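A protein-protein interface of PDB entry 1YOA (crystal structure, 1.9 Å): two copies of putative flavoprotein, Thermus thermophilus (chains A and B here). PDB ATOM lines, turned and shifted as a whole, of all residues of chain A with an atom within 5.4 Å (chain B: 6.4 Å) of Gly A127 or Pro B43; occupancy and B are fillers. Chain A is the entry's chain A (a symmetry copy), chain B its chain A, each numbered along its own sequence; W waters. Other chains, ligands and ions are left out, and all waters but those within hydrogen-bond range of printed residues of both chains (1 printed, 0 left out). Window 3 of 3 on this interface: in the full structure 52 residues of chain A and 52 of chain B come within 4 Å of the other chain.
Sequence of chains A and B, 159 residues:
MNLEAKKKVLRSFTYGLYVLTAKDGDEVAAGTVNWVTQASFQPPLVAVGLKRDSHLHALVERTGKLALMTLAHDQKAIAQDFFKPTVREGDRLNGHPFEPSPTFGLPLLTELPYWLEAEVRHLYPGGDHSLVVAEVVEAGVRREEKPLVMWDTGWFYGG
The backbone NH (N) of Gln B42 lies within hydrogen-bond range of the side-chain carboxylate (OD1) of Asp A128, 2.9 Å away. The side-chain hydroxyl of Ser B40 is in hydrogen-bond range of the side-chain carboxylate of Asp A128 (3.2 Å). The backbone NH (N) of Phe B41 is in hydrogen-bond range of the side-chain carboxylate (OD2) of Asp A128, at 3.0 Å.
The backbone carbonyl oxygen of Ser B40 is in hydrogen-bond range of the backbone NH of Leu B45 (3.4 Å). The side-chain hydroxyl (OG) of Ser B40 sits at hydrogen-bond distance from the backbone carbonyl oxygen (O) of Pro B43. The backbone NH of Ala B39 lies within hydrogen-bond range of the backbone carbonyl oxygen of Leu B45, at 2.9 Å. A ring nitrogen (ND1) of His A129 sits at hydrogen-bond distance from the side-chain carboxylate of Asp A128. The backbone NH (N) of Arg A52 is in hydrogen-bond range of the backbone carbonyl oxygen (O) of Asp A128, 2.8 Å away. O of Gln B42 sits at hydrogen-bond distance from OG of Ser B40.
CD of Pro B43 touches O of Gly A126, at 3.4 Å. Leu B45 touches Gly A126. OG of Ser B40 touches CA of Gly A127, 3.6 Å away. Gly A127 touches Gln B42 (CA to O, 3.4 Å). Gly A127 touches Pro B43. Ala B39 touches His A129 (O to CB, 3.4 Å). N of His A129 touches CB of Ser B40 (3.9 Å). Phe B41 touches His A129 (CE1 to CE1, 3.8 Å).
Of the printed residues of chain B, Gly A126 touches Pro B43 and Leu B45. Of chain B, only Ser B40 (3.6 Å), Gln B42 (3.4 Å) and Pro B43 (3.7 Å) come within 4 Å of Gly A127. Of the printed residues of chain B, His A129 touches Ala B39 (3.4 Å), Ser B40 (3.9 Å) and Phe B41 (3.8 Å). Of the printed residues of chain A, Ser B40 touches Gly A127, Asp A128 and His A129. Of the printed residues of chain A, Phe B41 touches Asp A128 and His A129. Of the printed residues of chain A, Gln B42 touches Gly A127 and Asp A128. Of the printed residues of chain A, Pro B43 touches Gly A126 and Gly A127. The nearest residue of chain A that does not touch Pro B43 is Asp A128 (4.9 Å).
Of the 7 printed residues of chain A, 4 touch a printed residue of chain B. Printed residues of chain A that touch a printed residue of chain B: Gly A126, Gly A127, Asp A128 and His A129. Along chain A the printed residues that touch a printed residue of chain B span positions 126 to 129. Printed residues of chain B that touch a printed residue of chain A: Ala B39, Ser B40, Phe B41, Gln B42, Pro B43 and Leu B45. Among the printed residues, 11 pairs touch across the chains. Among the printed residues, no Asp or Glu carboxylate lies within 4 Å of a Lys or Arg side-chain nitrogen of the other chain.
No position is printed for both chains.
Water W1 lies within hydrogen-bond range of O of His A129 (2.8 Å), O of Ala B39 (3.1 Å) and N of Gly A126 (3.2 Å).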
ATOM      1  N   ARG A  52       2.688  27.369   4.688  1.00  0.00           N
ATOM      2  CA  ARG A  52       2.749  26.896   3.318  1.00  0.00           C
ATOM      3  C   ARG A  52       1.897  27.807   2.419  1.00  0.00           C
ATOM      4  O   ARG A  52       2.277  28.080   1.281  1.00  0.00           O
ATOM      5  CB  ARG A  52       2.267  25.435   3.238  1.00  0.00           C
ATOM      6  CG  ARG A  52       1.788  24.984   1.854  1.00  0.00           C
ATOM      7  CD  ARG A  52       1.767  23.459   1.649  1.00  0.00           C
ATOM      8  NE  ARG A  52       3.125  22.928   1.719  1.00  0.00           N
ATOM      9  CZ  ARG A  52       4.062  23.079   0.782  1.00  0.00           C
ATOM     10  NH1 ARG A  52       3.810  23.701  -0.365  1.00  0.00           N
ATOM     11  NH2 ARG A  52       5.276  22.582   0.996  1.00  0.00           N
ATOM     12  N   PRO A 125       8.698  19.903   3.902  1.00  0.00           N
ATOM     13  CA  PRO A 125       7.263  20.229   3.882  1.00  0.00           C
ATOM     14  C   PRO A 125       6.443  19.392   4.862  1.00  0.00           C
ATOM     15  O   PRO A 125       5.659  18.505   4.474  1.00  0.00           O
ATOM     16  CB  PRO A 125       6.876  19.939   2.417  1.00  0.00           C
ATOM     17  CG  PRO A 125       7.802  18.831   1.999  1.00  0.00           C
ATOM     18  CD  PRO A 125       9.075  19.006   2.785  1.00  0.00           C
ATOM     19  N   GLY A 126       6.577  19.688   6.152  1.00  0.00           N
ATOM     20  CA  GLY A 126       6.038  18.819   7.178  1.00  0.00           C
ATOM     21  C   GLY A 126       4.553  18.861   7.415  1.00  0.00           C
ATOM     22  O   GLY A 126       3.975  17.884   7.885  1.00  0.00           O
ATOM     23  N   GLY A 127       3.928  20.008   7.142  1.00  0.00           N
ATOM     24  CA  GLY A 127       2.519  20.173   7.430  1.00  0.00           C
ATOM     25  C   GLY A 127       2.027  21.498   6.894  1.00  0.00           C
ATOM     26  O   GLY A 127       2.442  21.935   5.810  1.00  0.00           O
ATOM     27  N   ASP A 128       1.165  22.150   7.656  1.00  0.00           N
ATOM     28  CA  ASP A 128       0.666  23.462   7.246  1.00  0.00           C
ATOM     29  C   ASP A 128       1.786  24.518   7.191  1.00  0.00           C
ATOM     30  O   ASP A 128       1.596  25.567   6.605  1.00  0.00           O
ATOM     31  CB  ASP A 128      -0.530  23.926   8.084  1.00  0.00           C
ATOM     32  CG  ASP A 128      -0.281  23.895   9.573  1.00  0.00           C
ATOM     33  OD1 ASP A 128      -1.254  23.650  10.324  1.00  0.00           O
ATOM     34  OD2 ASP A 128       0.830  24.133  10.112  1.00  0.00           O
ATOM     35  N   HIS A 129       2.940  24.223   7.797  1.00  0.00           N
ATOM     36  CA  HIS A 129       4.157  25.035   7.657  1.00  0.00           C
ATOM     37  C   HIS A 129       5.259  24.143   7.118  1.00  0.00           C
ATOM     38  O   HIS A 129       5.294  22.928   7.430  1.00  0.00           O
ATOM     39  CB  HIS A 129       4.601  25.599   9.018  1.00  0.00           C
ATOM     40  CG  HIS A 129       3.718  26.675   9.559  1.00  0.00           C
ATOM     41  ND1 HIS A 129       2.390  26.462   9.872  1.00  0.00           N
ATOM     42  CD2 HIS A 129       3.975  27.968   9.876  1.00  0.00           C
ATOM     43  CE1 HIS A 129       1.866  27.582  10.331  1.00  0.00           C
ATOM     44  NE2 HIS A 129       2.810  28.510  10.356  1.00  0.00           N
ATOM     45  N   SER A 130       6.135  24.709   6.302  1.00  0.00           N
ATOM     46  CA  SER A 130       7.378  24.070   5.935  1.00  0.00           C
ATOM     47  C   SER A 130       8.481  24.540   6.876  1.00  0.00           C
ATOM     48  O   SER A 130       8.479  25.677   7.304  1.00  0.00           O
ATOM     49  CB  SER A 130       7.768  24.385   4.503  1.00  0.00           C
ATOM     50  OG  SER A 130       6.743  24.040   3.597  1.00  0.00           O
ATOM     51  N   GLN B  38       8.083  25.187  17.463  1.00  0.00           N
ATOM     52  CA  GLN B  38       7.006  24.482  16.780  1.00  0.00           C
ATOM     53  C   GLN B  38       7.245  24.648  15.246  1.00  0.00           C
ATOM     54  O   GLN B  38       7.876  25.626  14.800  1.00  0.00           O
ATOM     55  CB  GLN B  38       5.647  25.002  17.282  1.00  0.00           C
ATOM     56  CG  GLN B  38       4.463  24.287  16.685  1.00  0.00           C
ATOM     57  CD  GLN B  38       3.139  24.523  17.357  1.00  0.00           C
ATOM     58  OE1 GLN B  38       2.100  24.003  16.845  1.00  0.00           O
ATOM     59  NE2 GLN B  38       3.105  25.318  18.392  1.00  0.00           N
ATOM     60  N   ALA B  39       6.803  23.673  14.448  1.00  0.00           N
ATOM     61  CA  ALA B  39       7.035  23.652  13.007  1.00  0.00           C
ATOM     62  C   ALA B  39       5.778  23.312  12.144  1.00  0.00           C
ATOM     63  O   ALA B  39       5.914  23.094  10.966  1.00  0.00           O
ATOM     64  CB  ALA B  39       8.158  22.714  12.686  1.00  0.00           C
ATOM     65  N   SER B  40       4.615  23.256  12.772  1.00  0.00           N
ATOM     66  CA  SER B  40       3.290  23.128  12.096  1.00  0.00           C
ATOM     67  C   SER B  40       2.220  22.943  13.211  1.00  0.00           C
ATOM     68  O   SER B  40       2.530  22.500  14.305  1.00  0.00           O
ATOM     69  CB  SER B  40       3.346  22.057  10.970  1.00  0.00           C
ATOM     70  OG  SER B  40       2.155  21.308  10.876  1.00  0.00           O
ATOM     71  N   PHE B  41       0.984  23.388  12.973  1.00  0.00           N
ATOM     72  CA  PHE B  41      -0.118  23.145  13.869  1.00  0.00           C
ATOM     73  C   PHE B  41      -0.677  21.757  13.558  1.00  0.00           C
ATOM     74  O   PHE B  41      -0.954  20.981  14.474  1.00  0.00           O
ATOM     75  CB  PHE B  41      -1.233  24.196  13.653  1.00  0.00           C
ATOM     76  CG  PHE B  41      -0.839  25.597  14.046  1.00  0.00           C
ATOM     77  CD1 PHE B  41      -0.628  26.567  13.080  1.00  0.00           C
ATOM     78  CD2 PHE B  41      -0.678  25.944  15.378  1.00  0.00           C
ATOM     79  CE1 PHE B  41      -0.298  27.895  13.448  1.00  0.00           C
ATOM     80  CE2 PHE B  41      -0.320  27.247  15.750  1.00  0.00           C
ATOM     81  CZ  PHE B  41      -0.146  28.233  14.758  1.00  0.00           C
ATOM     82  N   GLN B  42      -0.849  21.476  12.264  1.00  0.00           N
ATOM     83  CA  GLN B  42      -1.261  20.152  11.774  1.00  0.00           C
ATOM     84  C   GLN B  42      -0.243  19.657  10.760  1.00  0.00           C
ATOM     85  O   GLN B  42       0.045  20.340   9.756  1.00  0.00           O
ATOM     86  CB  GLN B  42      -2.668  20.222  11.141  1.00  0.00           C
ATOM     87  CG  GLN B  42      -3.047  18.983  10.320  1.00  0.00           C
ATOM     88  CD  GLN B  42      -4.475  19.046   9.781  1.00  0.00           C
ATOM     89  OE1 GLN B  42      -5.045  20.146   9.612  1.00  0.00           O
ATOM     90  NE2 GLN B  42      -5.055  17.876   9.497  1.00  0.00           N
ATOM     91  N   PRO B  43       0.394  18.519  11.014  1.00  0.00           N
ATOM     92  CA  PRO B  43       0.394  17.821  12.306  1.00  0.00           C
ATOM     93  C   PRO B  43       1.118  18.674  13.339  1.00  0.00           C
ATOM     94  O   PRO B  43       1.755  19.656  12.927  1.00  0.00           O
ATOM     95  CB  PRO B  43       1.210  16.548  12.026  1.00  0.00           C
ATOM     96  CG  PRO B  43       1.590  16.566  10.619  1.00  0.00           C
ATOM     97  CD  PRO B  43       1.273  17.884  10.030  1.00  0.00           C
ATOM     98  N   PRO B  44       0.996  18.361  14.631  1.00  0.00           N
ATOM     99  CA  PRO B  44       1.700  19.131  15.656  1.00  0.00           C
ATOM    100  C   PRO B  44       3.177  18.750  15.681  1.00  0.00           C
ATOM    101  O   PRO B  44       3.561  17.780  16.311  1.00  0.00           O
ATOM    102  CB  PRO B  44       0.976  18.756  16.939  1.00  0.00           C
ATOM    103  CG  PRO B  44       0.430  17.358  16.681  1.00  0.00           C
ATOM    104  CD  PRO B  44       0.170  17.288  15.211  1.00  0.00           C
ATOM    105  N   LEU B  45       3.995  19.533  14.986  1.00  0.00           N
ATOM    106  CA  LEU B  45       5.415  19.251  14.857  1.00  0.00           C
ATOM    107  C   LEU B  45       6.273  20.160  15.717  1.00  0.00           C
ATOM    108  O   LEU B  45       5.984  21.332  15.859  1.00  0.00           O
ATOM    109  CB  LEU B  45       5.837  19.415  13.401  1.00  0.00           C
ATOM    110  CG  LEU B  45       5.132  18.503  12.386  1.00  0.00           C
ATOM    111  CD1 LEU B  45       5.604  18.862  11.036  1.00  0.00           C
ATOM    112  CD2 LEU B  45       5.376  17.024  12.669  1.00  0.00           C
ATOM    113  N   ARG B 121       9.861  12.431  12.636  1.00  0.00           N
ATOM    114  CA  ARG B 121       9.316  12.351  11.279  1.00  0.00           C
ATOM    115  C   ARG B 121      10.376  12.616  10.240  1.00  0.00           C
ATOM    116  O   ARG B 121      10.273  12.137   9.103  1.00  0.00           O
ATOM    117  CB  ARG B 121       8.187  13.370  11.097  1.00  0.00           C
ATOM    118  CG  ARG B 121       6.945  13.030  11.846  1.00  0.00           C
ATOM    119  CD  ARG B 121       6.175  11.816  11.275  1.00  0.00           C
ATOM    120  NE  ARG B 121       5.070  11.475  12.162  1.00  0.00           N
ATOM    121  CZ  ARG B 121       4.976  10.360  12.878  1.00  0.00           C
ATOM    122  NH1 ARG B 121       5.903   9.416  12.794  1.00  0.00           N
ATOM    123  NH2 ARG B 121       3.929  10.179  13.678  1.00  0.00           N
ATOM    124  N   GLU B 135       6.672  14.674  15.594  1.00  0.00           N
ATOM    125  CA  GLU B 135       5.247  14.903  15.798  1.00  0.00           C
ATOM    126  C   GLU B 135       4.867  14.573  17.241  1.00  0.00           C
ATOM    127  O   GLU B 135       5.241  13.522  17.768  1.00  0.00           O
ATOM    128  CB  GLU B 135       4.419  14.069  14.806  1.00  0.00           C
ATOM    129  CG  GLU B 135       2.922  14.233  14.999  1.00  0.00           C
ATOM    130  CD  GLU B 135       2.073  13.583  13.911  1.00  0.00           C
ATOM    131  OE1 GLU B 135       2.617  13.041  12.930  1.00  0.00           O
ATOM    132  OE2 GLU B 135       0.836  13.648  14.044  1.00  0.00           O
ATOM    133  N   VAL B 136       4.123  15.470  17.876  1.00  0.00           N
ATOM    134  CA  VAL B 136       3.705  15.290  19.247  1.00  0.00           C
ATOM    135  C   VAL B 136       2.656  14.162  19.269  1.00  0.00           C
ATOM    136  O   VAL B 136       1.682  14.211  18.529  1.00  0.00           O
ATOM    137  CB  VAL B 136       3.137  16.583  19.843  1.00  0.00           C
ATOM    138  CG1 VAL B 136       2.597  16.356  21.240  1.00  0.00           C
ATOM    139  CG2 VAL B 136       4.183  17.676  19.864  1.00  0.00           C
HETATM  140  O   HOH W   1       7.280  21.392   8.759  1.00  0.00           O
